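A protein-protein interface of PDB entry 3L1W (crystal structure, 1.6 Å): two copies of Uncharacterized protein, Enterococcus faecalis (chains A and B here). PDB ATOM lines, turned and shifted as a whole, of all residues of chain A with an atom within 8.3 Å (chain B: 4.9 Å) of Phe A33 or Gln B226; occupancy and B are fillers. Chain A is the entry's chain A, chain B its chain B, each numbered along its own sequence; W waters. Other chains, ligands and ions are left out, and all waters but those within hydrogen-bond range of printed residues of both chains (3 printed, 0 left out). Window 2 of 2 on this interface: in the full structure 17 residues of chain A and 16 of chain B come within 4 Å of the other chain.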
ATOM      1  N   ALA A  26     -17.517  11.056  -7.766  1.00  0.00           N
ATOM      2  CA  ALA A  26     -16.490  10.485  -6.910  1.00  0.00           C
ATOM      3  C   ALA A  26     -16.989   9.219  -6.224  1.00  0.00           C
ATOM      4  O   ALA A  26     -16.269   8.228  -6.138  1.00  0.00           O
ATOM      5  CB  ALA A  26     -16.020  11.509  -5.879  1.00  0.00           C
ATOM      6  N   VAL A  27     -18.224   9.253  -5.726  1.00  0.00           N
ATOM      7  CA  VAL A  27     -18.796   8.071  -5.094  1.00  0.00           C
ATOM      8  C   VAL A  27     -18.937   6.918  -6.091  1.00  0.00           C
ATOM      9  O   VAL A  27     -18.556   5.784  -5.806  1.00  0.00           O
ATOM     10  CB  VAL A  27     -20.166   8.392  -4.440  1.00  0.00           C
ATOM     11  CG1 VAL A  27     -20.915   7.105  -4.058  1.00  0.00           C
ATOM     12  CG2 VAL A  27     -19.967   9.293  -3.236  1.00  0.00           C
ATOM     13  N   CYS A  28     -19.486   7.207  -7.265  1.00  0.00           N
ATOM     14  CA  CYS A  28     -19.706   6.150  -8.247  1.00  0.00           C
ATOM     15  C   CYS A  28     -18.397   5.598  -8.815  1.00  0.00           C
ATOM     16  O   CYS A  28     -18.282   4.399  -9.081  1.00  0.00           O
ATOM     17  CB  CYS A  28     -20.620   6.639  -9.368  1.00  0.00           C
ATOM     18  SG  CYS A  28     -22.327   6.903  -8.811  1.00  0.00           S
ATOM     19  N   GLN A  29     -17.410   6.469  -9.009  1.00  0.00           N
ATOM     20  CA  GLN A  29     -16.114   6.019  -9.509  1.00  0.00           C
ATOM     21  C   GLN A  29     -15.402   5.158  -8.475  1.00  0.00           C
ATOM     22  O   GLN A  29     -14.696   4.212  -8.824  1.00  0.00           O
ATOM     23  CB  GLN A  29     -15.250   7.218  -9.911  1.00  0.00           C
ATOM     24  CG  GLN A  29     -15.704   7.833 -11.224  1.00  0.00           C
ATOM     25  CD  GLN A  29     -15.107   9.194 -11.451  1.00  0.00           C
ATOM     26  OE1 GLN A  29     -14.200   9.608 -10.733  1.00  0.00           O
ATOM     27  NE2 GLN A  29     -15.623   9.912 -12.447  1.00  0.00           N
ATOM     28  N   LEU A  30     -15.584   5.482  -7.200  1.00  0.00           N
ATOM     29  CA  LEU A  30     -14.991   4.674  -6.144  1.00  0.00           C
ATOM     30  C   LEU A  30     -15.565   3.266  -6.205  1.00  0.00           C
ATOM     31  O   LEU A  30     -14.825   2.281  -6.184  1.00  0.00           O
ATOM     32  CB  LEU A  30     -15.245   5.318  -4.776  1.00  0.00           C
ATOM     33  CG  LEU A  30     -14.631   4.661  -3.530  1.00  0.00           C
ATOM     34  CD1 LEU A  30     -14.585   5.673  -2.393  1.00  0.00           C
ATOM     35  CD2 LEU A  30     -15.392   3.404  -3.082  1.00  0.00           C
ATOM     36  N   ILE A  31     -16.892   3.182  -6.276  1.00  0.00           N
ATOM     37  CA  ILE A  31     -17.574   1.898  -6.385  1.00  0.00           C
ATOM     38  C   ILE A  31     -17.088   1.123  -7.614  1.00  0.00           C
ATOM     39  O   ILE A  31     -16.762  -0.064  -7.521  1.00  0.00           O
ATOM     40  CB  ILE A  31     -19.110   2.104  -6.402  1.00  0.00           C
ATOM     41  CG1 ILE A  31     -19.561   2.651  -5.042  1.00  0.00           C
ATOM     42  CG2 ILE A  31     -19.827   0.801  -6.761  1.00  0.00           C
ATOM     43  CD1 ILE A  31     -20.976   3.243  -5.028  1.00  0.00           C
ATOM     44  N   ASN A  32     -17.005   1.786  -8.762  1.00  0.00           N
ATOM     45  CA  ASN A  32     -16.572   1.075  -9.970  1.00  0.00           C
ATOM     46  C   ASN A  32     -15.150   0.548  -9.868  1.00  0.00           C
ATOM     47  O   ASN A  32     -14.852  -0.549 -10.351  1.00  0.00           O
ATOM     48  CB  ASN A  32     -16.680   1.965 -11.199  1.00  0.00           C
ATOM     49  CG  ASN A  32     -18.113   2.181 -11.627  1.00  0.00           C
ATOM     50  OD1 ASN A  32     -19.018   1.452 -11.216  1.00  0.00           O
ATOM     51  ND2 ASN A  32     -18.325   3.181 -12.469  1.00  0.00           N
ATOM     52  N   PHE A  33     -14.284   1.344  -9.245  1.00  0.00           N
ATOM     53  CA  PHE A  33     -12.873   0.992  -9.117  1.00  0.00           C
ATOM     54  C   PHE A  33     -12.647  -0.189  -8.179  1.00  0.00           C
ATOM     55  O   PHE A  33     -11.891  -1.103  -8.497  1.00  0.00           O
ATOM     56  CB  PHE A  33     -12.039   2.191  -8.665  1.00  0.00           C
ATOM     57  CG  PHE A  33     -10.599   1.850  -8.400  1.00  0.00           C
ATOM     58  CD1 PHE A  33      -9.722   1.626  -9.446  1.00  0.00           C
ATOM     59  CD2 PHE A  33     -10.132   1.742  -7.100  1.00  0.00           C
ATOM     60  CE1 PHE A  33      -8.383   1.302  -9.201  1.00  0.00           C
ATOM     61  CE2 PHE A  33      -8.793   1.419  -6.841  1.00  0.00           C
ATOM     62  CZ  PHE A  33      -7.930   1.196  -7.888  1.00  0.00           C
ATOM     63  N   HIS A  34     -13.297  -0.170  -7.024  1.00  0.00           N
ATOM     64  CA  HIS A  34     -13.135  -1.279  -6.091  1.00  0.00           C
ATOM     65  C   HIS A  34     -13.818  -2.568  -6.559  1.00  0.00           C
ATOM     66  O   HIS A  34     -13.315  -3.671  -6.283  1.00  0.00           O
ATOM     67  CB  HIS A  34     -13.486  -0.846  -4.667  1.00  0.00           C
ATOM     68  CG  HIS A  34     -12.522   0.166  -4.132  1.00  0.00           C
ATOM     69  ND1 HIS A  34     -11.309  -0.191  -3.581  1.00  0.00           N
ATOM     70  CD2 HIS A  34     -12.551   1.521  -4.135  1.00  0.00           C
ATOM     71  CE1 HIS A  34     -10.647   0.901  -3.238  1.00  0.00           C
ATOM     72  NE2 HIS A  34     -11.374   1.953  -3.572  1.00  0.00           N
ATOM     73  N   ASP A  35     -14.936  -2.420  -7.272  1.00  0.00           N
ATOM     74  CA  ASP A  35     -15.464  -3.489  -8.113  1.00  0.00           C
ATOM     75  C   ASP A  35     -15.735  -4.780  -7.337  1.00  0.00           C
ATOM     76  O   ASP A  35     -15.406  -5.878  -7.797  1.00  0.00           O
ATOM     77  CB  ASP A  35     -14.460  -3.757  -9.239  1.00  0.00           C
ATOM     78  CG  ASP A  35     -15.026  -4.600 -10.360  1.00  0.00           C
ATOM     79  OD1 ASP A  35     -16.227  -4.491 -10.661  1.00  0.00           O
ATOM     80  OD2 ASP A  35     -14.236  -5.353 -10.968  1.00  0.00           O
ATOM     81  N   TRP A  36     -16.343  -4.643  -6.165  1.00  0.00           N
ATOM     82  CA  TRP A  36     -16.680  -5.797  -5.330  1.00  0.00           C
ATOM     83  C   TRP A  36     -17.727  -6.689  -5.995  1.00  0.00           C
ATOM     84  O   TRP A  36     -18.350  -6.285  -6.982  1.00  0.00           O
ATOM     85  CB  TRP A  36     -17.242  -5.320  -3.988  1.00  0.00           C
ATOM     86  CG  TRP A  36     -16.454  -4.221  -3.310  1.00  0.00           C
ATOM     87  CD1 TRP A  36     -15.285  -4.352  -2.605  1.00  0.00           C
ATOM     88  CD2 TRP A  36     -16.814  -2.836  -3.232  1.00  0.00           C
ATOM     89  NE1 TRP A  36     -14.890  -3.121  -2.112  1.00  0.00           N
ATOM     90  CE2 TRP A  36     -15.814  -2.180  -2.483  1.00  0.00           C
ATOM     91  CE3 TRP A  36     -17.878  -2.081  -3.740  1.00  0.00           C
ATOM     92  CZ2 TRP A  36     -15.851  -0.813  -2.223  1.00  0.00           C
ATOM     93  CZ3 TRP A  36     -17.919  -0.728  -3.478  1.00  0.00           C
ATOM     94  CH2 TRP A  36     -16.915  -0.106  -2.721  1.00  0.00           C
ATOM     95  N   TYR A  55     -24.393   5.452 -13.263  1.00  0.00           N
ATOM     96  CA  TYR A  55     -22.956   5.733 -13.241  1.00  0.00           C
ATOM     97  C   TYR A  55     -22.075   4.663 -12.606  1.00  0.00           C
ATOM     98  O   TYR A  55     -20.858   4.807 -12.589  1.00  0.00           O
ATOM     99  CB  TYR A  55     -22.693   7.096 -12.583  1.00  0.00           C
ATOM    100  CG  TYR A  55     -23.283   8.232 -13.375  1.00  0.00           C
ATOM    101  CD1 TYR A  55     -22.681   8.670 -14.539  1.00  0.00           C
ATOM    102  CD2 TYR A  55     -24.448   8.864 -12.959  1.00  0.00           C
ATOM    103  CE1 TYR A  55     -23.219   9.708 -15.275  1.00  0.00           C
ATOM    104  CE2 TYR A  55     -24.995   9.908 -13.689  1.00  0.00           C
ATOM    105  CZ  TYR A  55     -24.373  10.320 -14.848  1.00  0.00           C
ATOM    106  OH  TYR A  55     -24.908  11.345 -15.592  1.00  0.00           O
ATOM    107  N   THR A  56     -22.669   3.599 -12.079  1.00  0.00           N
ATOM    108  CA  THR A  56     -21.870   2.440 -11.701  1.00  0.00           C
ATOM    109  C   THR A  56     -22.168   1.289 -12.646  1.00  0.00           C
ATOM    110  O   THR A  56     -23.145   1.311 -13.414  1.00  0.00           O
ATOM    111  CB  THR A  56     -22.090   1.953 -10.232  1.00  0.00           C
ATOM    112  OG1 THR A  56     -23.289   1.169 -10.162  1.00  0.00           O
ATOM    113  CG2 THR A  56     -22.170   3.127  -9.250  1.00  0.00           C
ATOM    114  N   THR A  57     -21.321   0.272 -12.566  1.00  0.00           N
ATOM    115  CA  THR A  57     -21.430  -0.901 -13.417  1.00  0.00           C
ATOM    116  C   THR A  57     -22.347  -1.964 -12.804  1.00  0.00           C
ATOM    117  O   THR A  57     -22.553  -3.017 -13.399  1.00  0.00           O
ATOM    118  CB  THR A  57     -20.045  -1.521 -13.617  1.00  0.00           C
ATOM    119  OG1 THR A  57     -19.479  -1.820 -12.336  1.00  0.00           O
ATOM    120  CG2 THR A  57     -19.126  -0.520 -14.329  1.00  0.00           C
ATOM    121  N   PHE A  58     -22.917  -1.672 -11.639  1.00  0.00           N
ATOM    122  CA  PHE A  58     -23.642  -2.686 -10.861  1.00  0.00           C
ATOM    123  C   PHE A  58     -25.144  -2.786 -11.118  1.00  0.00           C
ATOM    124  O   PHE A  58     -25.799  -1.809 -11.468  1.00  0.00           O
ATOM    125  CB  PHE A  58     -23.459  -2.423  -9.363  1.00  0.00           C
ATOM    126  CG  PHE A  58     -22.094  -2.741  -8.857  1.00  0.00           C
ATOM    127  CD1 PHE A  58     -21.053  -1.855  -9.040  1.00  0.00           C
ATOM    128  CD2 PHE A  58     -21.850  -3.930  -8.188  1.00  0.00           C
ATOM    129  CE1 PHE A  58     -19.772  -2.152  -8.569  1.00  0.00           C
ATOM    130  CE2 PHE A  58     -20.580  -4.237  -7.711  1.00  0.00           C
ATOM    131  CZ  PHE A  58     -19.533  -3.347  -7.909  1.00  0.00           C
ATOM    132  N   LYS A  82     -20.827 -12.334 -10.949  1.00  0.00           N
ATOM    133  CA  LYS A  82     -20.184 -12.842  -9.738  1.00  0.00           C
ATOM    134  C   LYS A  82     -21.185 -13.457  -8.761  1.00  0.00           C
ATOM    135  O   LYS A  82     -20.909 -14.486  -8.134  1.00  0.00           O
ATOM    136  CB  LYS A  82     -19.408 -11.716  -9.042  1.00  0.00           C
ATOM    137  CG  LYS A  82     -18.251 -11.167  -9.883  1.00  0.00           C
ATOM    138  CD  LYS A  82     -17.496 -10.081  -9.147  1.00  0.00           C
ATOM    139  CE  LYS A  82     -16.297  -9.579  -9.964  1.00  0.00           C
ATOM    140  NZ  LYS A  82     -15.659  -8.389  -9.320  1.00  0.00           N
ATOM    141  N   LEU A 230     -11.705   2.062   3.573  1.00  0.00           N
ATOM    142  CA  LEU A 230     -11.097   2.666   2.384  1.00  0.00           C
ATOM    143  C   LEU A 230     -11.084   4.192   2.479  1.00  0.00           C
ATOM    144  O   LEU A 230     -12.128   4.820   2.590  1.00  0.00           O
ATOM    145  CB  LEU A 230     -11.872   2.221   1.135  1.00  0.00           C
ATOM    146  CG  LEU A 230     -11.977   0.696   0.999  1.00  0.00           C
ATOM    147  CD1 LEU A 230     -12.817   0.309  -0.208  1.00  0.00           C
ATOM    148  CD2 LEU A 230     -10.575   0.068   0.904  1.00  0.00           C
ATOM    149  N   ASP A 232     -10.122   6.485   0.294  1.00  0.00           N
ATOM    150  CA  ASP A 232     -10.140   7.195  -0.989  1.00  0.00           C
ATOM    151  C   ASP A 232     -10.627   8.626  -0.813  1.00  0.00           C
ATOM    152  O   ASP A 232     -11.630   8.880  -0.130  1.00  0.00           O
ATOM    153  CB  ASP A 232     -11.088   6.510  -1.973  1.00  0.00           C
ATOM    154  CG  ASP A 232     -10.738   5.064  -2.230  1.00  0.00           C
ATOM    155  OD1 ASP A 232     -10.336   4.358  -1.278  1.00  0.00           O
ATOM    156  OD2 ASP A 232     -10.896   4.624  -3.391  1.00  0.00           O
ATOM    157  N   GLU A 246     -14.831  -2.752   3.588  1.00  0.00           N
ATOM    158  CA  GLU A 246     -14.871  -3.958   2.779  1.00  0.00           C
ATOM    159  C   GLU A 246     -14.340  -5.195   3.500  1.00  0.00           C
ATOM    160  O   GLU A 246     -13.632  -5.093   4.507  1.00  0.00           O
ATOM    161  CB  GLU A 246     -14.149  -3.740   1.446  1.00  0.00           C
ATOM    162  CG  GLU A 246     -12.643  -3.632   1.554  1.00  0.00           C
ATOM    163  CD  GLU A 246     -11.952  -3.839   0.205  1.00  0.00           C
ATOM    164  OE1 GLU A 246     -12.420  -3.293  -0.817  1.00  0.00           O
ATOM    165  OE2 GLU A 246     -10.938  -4.562   0.168  1.00  0.00           O
ATOM    166  N   ALA B 190      -7.226   4.420 -21.041  1.00  0.00           N
ATOM    167  CA  ALA B 190      -8.462   3.916 -20.473  1.00  0.00           C
ATOM    168  C   ALA B 190      -8.942   4.884 -19.405  1.00  0.00           C
ATOM    169  O   ALA B 190      -8.548   6.049 -19.402  1.00  0.00           O
ATOM    170  CB  ALA B 190      -8.250   2.514 -19.901  1.00  0.00           C
ATOM    171  N   THR B 191      -9.806   4.412 -18.517  1.00  0.00           N
ATOM    172  CA  THR B 191     -10.271   5.235 -17.414  1.00  0.00           C
ATOM    173  C   THR B 191      -9.190   5.306 -16.337  1.00  0.00           C
ATOM    174  O   THR B 191      -8.568   4.298 -16.009  1.00  0.00           O
ATOM    175  CB  THR B 191     -11.586   4.683 -16.822  1.00  0.00           C
ATOM    176  OG1 THR B 191     -12.557   4.548 -17.870  1.00  0.00           O
ATOM    177  CG2 THR B 191     -12.130   5.620 -15.760  1.00  0.00           C
ATOM    178  N   TYR B 193      -8.344   6.417 -12.357  1.00  0.00           N
ATOM    179  CA  TYR B 193      -8.939   6.695 -11.048  1.00  0.00           C
ATOM    180  C   TYR B 193      -7.917   7.400 -10.177  1.00  0.00           C
ATOM    181  O   TYR B 193      -6.749   7.013 -10.148  1.00  0.00           O
ATOM    182  CB  TYR B 193      -9.392   5.386 -10.389  1.00  0.00           C
ATOM    183  CG  TYR B 193     -10.066   5.562  -9.044  1.00  0.00           C
ATOM    184  CD1 TYR B 193     -11.268   6.242  -8.932  1.00  0.00           C
ATOM    185  CD2 TYR B 193      -9.503   5.022  -7.889  1.00  0.00           C
ATOM    186  CE1 TYR B 193     -11.890   6.398  -7.700  1.00  0.00           C
ATOM    187  CE2 TYR B 193     -10.112   5.174  -6.652  1.00  0.00           C
ATOM    188  CZ  TYR B 193     -11.304   5.858  -6.564  1.00  0.00           C
ATOM    189  OH  TYR B 193     -11.922   6.026  -5.348  1.00  0.00           O
ATOM    190  N   VAL B 224      -4.742  -1.797 -22.278  1.00  0.00           N
ATOM    191  CA  VAL B 224      -4.910  -1.219 -20.943  1.00  0.00           C
ATOM    192  C   VAL B 224      -6.396  -1.148 -20.577  1.00  0.00           C
ATOM    193  O   VAL B 224      -7.212  -0.647 -21.359  1.00  0.00           O
ATOM    194  CB  VAL B 224      -4.292   0.180 -20.881  1.00  0.00           C
ATOM    195  CG1 VAL B 224      -4.523   0.804 -19.496  1.00  0.00           C
ATOM    196  CG2 VAL B 224      -2.800   0.098 -21.194  1.00  0.00           C
ATOM    197  N   GLN B 225      -6.737  -1.661 -19.398  1.00  0.00           N
ATOM    198  CA  GLN B 225      -8.127  -1.708 -18.937  1.00  0.00           C
ATOM    199  C   GLN B 225      -8.485  -0.580 -17.996  1.00  0.00           C
ATOM    200  O   GLN B 225      -9.646  -0.172 -17.917  1.00  0.00           O
ATOM    201  CB  GLN B 225      -8.425  -3.029 -18.221  1.00  0.00           C
ATOM    202  CG  GLN B 225      -8.695  -4.190 -19.151  1.00  0.00           C
ATOM    203  CD  GLN B 225      -7.430  -4.801 -19.681  1.00  0.00           C
ATOM    204  OE1 GLN B 225      -7.190  -4.810 -20.890  1.00  0.00           O
ATOM    205  NE2 GLN B 225      -6.602  -5.320 -18.779  1.00  0.00           N
ATOM    206  N   GLN B 226      -7.484  -0.084 -17.279  1.00  0.00           N
ATOM    207  CA  GLN B 226      -7.704   0.885 -16.225  1.00  0.00           C
ATOM    208  C   GLN B 226      -6.362   1.293 -15.618  1.00  0.00           C
ATOM    209  O   GLN B 226      -5.398   0.523 -15.651  1.00  0.00           O
ATOM    210  CB  GLN B 226      -8.600   0.246 -15.168  1.00  0.00           C
ATOM    211  CG  GLN B 226      -8.648   0.934 -13.833  1.00  0.00           C
ATOM    212  CD  GLN B 226      -9.429   0.116 -12.831  1.00  0.00           C
ATOM    213  OE1 GLN B 226      -9.078   0.054 -11.659  1.00  0.00           O
ATOM    214  NE2 GLN B 226     -10.482  -0.543 -13.302  1.00  0.00           N
ATOM    215  N   THR B 227      -6.293   2.504 -15.081  1.00  0.00           N
ATOM    216  CA  THR B 227      -5.114   2.924 -14.337  1.00  0.00           C
ATOM    217  C   THR B 227      -5.593   3.664 -13.095  1.00  0.00           C
ATOM    218  O   THR B 227      -6.752   4.090 -13.028  1.00  0.00           O
ATOM    219  CB  THR B 227      -4.186   3.846 -15.154  1.00  0.00           C
ATOM    220  OG1 THR B 227      -4.943   4.959 -15.647  1.00  0.00           O
ATOM    221  CG2 THR B 227      -3.566   3.075 -16.338  1.00  0.00           C
ATOM    222  N   ALA B 228      -4.709   3.805 -12.113  1.00  0.00           N
ATOM    223  CA  ALA B 228      -5.063   4.541 -10.900  1.00  0.00           C
ATOM    224  C   ALA B 228      -3.840   5.070 -10.177  1.00  0.00           C
ATOM    225  O   ALA B 228      -2.784   4.448 -10.193  1.00  0.00           O
ATOM    226  CB  ALA B 228      -5.883   3.652  -9.953  1.00  0.00           C
ATOM    227  N   LEU B 230      -2.918   5.872  -6.294  1.00  0.00           N
ATOM    228  CA  LEU B 230      -3.501   5.406  -5.037  1.00  0.00           C
ATOM    229  C   LEU B 230      -3.198   6.371  -3.888  1.00  0.00           C
ATOM    230  O   LEU B 230      -2.037   6.606  -3.551  1.00  0.00           O
ATOM    231  CB  LEU B 230      -2.977   3.999  -4.715  1.00  0.00           C
ATOM    232  CG  LEU B 230      -3.170   2.972  -5.837  1.00  0.00           C
ATOM    233  CD1 LEU B 230      -2.579   1.613  -5.448  1.00  0.00           C
ATOM    234  CD2 LEU B 230      -4.659   2.819  -6.210  1.00  0.00           C
ATOM    235  N   GLU B 246      -0.879   2.402 -10.457  1.00  0.00           N
ATOM    236  CA  GLU B 246      -1.157   1.039 -10.888  1.00  0.00           C
ATOM    237  C   GLU B 246      -1.868   1.001 -12.228  1.00  0.00           C
ATOM    238  O   GLU B 246      -2.425   2.000 -12.676  1.00  0.00           O
ATOM    239  CB  GLU B 246      -1.936   0.270  -9.818  1.00  0.00           C
ATOM    240  CG  GLU B 246      -3.374   0.716  -9.629  1.00  0.00           C
ATOM    241  CD  GLU B 246      -4.233  -0.339  -8.911  1.00  0.00           C
ATOM    242  OE1 GLU B 246      -3.784  -0.920  -7.903  1.00  0.00           O
ATOM    243  OE2 GLU B 246      -5.371  -0.591  -9.357  1.00  0.00           O
ATOM    244  N   ALA B 247      -1.797  -0.142 -12.895  1.00  0.00           N
ATOM    245  CA  ALA B 247      -2.516  -0.336 -14.142  1.00  0.00           C
ATOM    246  C   ALA B 247      -3.051  -1.751 -14.190  1.00  0.00           C
ATOM    247  O   ALA B 247      -2.492  -2.658 -13.586  1.00  0.00           O
ATOM    248  CB  ALA B 247      -1.605  -0.090 -15.335  1.00  0.00           C
ATOM    249  N   GLU B 248      -4.150  -1.928 -14.903  1.00  0.00           N
ATOM    250  CA  GLU B 248      -4.633  -3.256 -15.244  1.00  0.00           C
ATOM    251  C   GLU B 248      -4.409  -3.453 -16.739  1.00  0.00           C
ATOM    252  O   GLU B 248      -4.879  -2.656 -17.553  1.00  0.00           O
ATOM    253  CB  GLU B 248      -6.106  -3.422 -14.873  1.00  0.00           C
ATOM    254  CG  GLU B 248      -6.583  -4.860 -15.027  1.00  0.00           C
ATOM    255  CD  GLU B 248      -8.036  -5.046 -14.675  1.00  0.00           C
ATOM    256  OE1 GLU B 248      -8.698  -4.058 -14.288  1.00  0.00           O
ATOM    257  OE2 GLU B 248      -8.513  -6.191 -14.788  1.00  0.00           O
HETATM  258  O   HOH W   1     -13.575   8.573  -5.439  1.00  0.00           O
HETATM  259  O   HOH W   2     -10.621  -1.858 -10.623  1.00  0.00           O
HETATM  260  O   HOH W   3     -12.860  -1.482 -12.158  1.00  0.00           O
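O of Gln A29 touches CE1 of Tyr B193 (3.7 Å).
Tyr B193 touches Leu A30 (OH to CB, 3.4 Å).
Phe A33 touches Tyr B193 (CG to CD2, 3.4 Å).
Phe A33 touches Gln B226 (CD1 to OE1, 2.8 Å).
Phe A33 touches Ala B228.
Phe A33 touches Glu B246.
Of the printed residues of chain B, Leu A30 touches Tyr B193 (3.4 Å).
Of the printed residues of chain B, Phe A33 touches Tyr B193, Gln B226, Ala B228 and Glu B246.
Of the printed residues of chain A, Tyr B193 touches Gln A29, Leu A30, Phe A33 and Asp A232.
Thr B227 touches none of the printed residues of chain A.
Of the printed residues of chain A, Ala B228 touches Phe A33.
The nearest printed residue of chain B that does not touch Phe A33 is Leu B230 (4.02 Å).
Water W2 bridges O of Phe A33 (2.6 Å) and OE1 of Gln B226 (2.7 Å).
Water W3 lies within hydrogen-bond range of NE2 of Gln B226 (2.8 Å) and O of Asn A32 (2.8 Å).
Water W1 lies within hydrogen-bond range of the backbone carbonyl oxygen (O) of Ala A26 (2.8 Å) and the side-chain hydroxyl (OH) of Tyr B193 (3.0 Å).
Printed residues of chain B that touch a printed residue of chain A: Tyr B193, Gln B226, Ala B228 and Glu B246.
Along chain B the printed residues that touch a printed residue of chain A span positions 193 to 246.
Hydrophobic or aromatic side chains of chain A within 4 Å of the printed part of chain B: Leu A30 and Phe A33.
Among the printed residues, no Asp or Glu carboxylate lies within 4 Å of a Lys or Arg side-chain nitrogen of the other chain.
A ring nitrogen (NE2) of His A34 sits at hydrogen-bond distance from the side-chain carboxylate of Asp A232 (2.7 Å).
The backbone carbonyl oxygen of Thr B227 lies within hydrogen-bond range of the backbone NH of Tyr B193.
O of Gln B226 lies within hydrogen-bond range of N of Glu B248 (2.9 Å).
The backbone carbonyl oxygen (O) of Ala B228 lies within hydrogen-bond range of the backbone NH (N) of Glu B246 (2.8 Å).
OD2 of Asp A232 sits at hydrogen-bond distance from OH of Tyr B193, at 2.6 Å.
2 positions are printed for both chains.
Of the 7 pairs that touch across the chains among the printed residues, none has its exchanged pair printed and touching as well.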
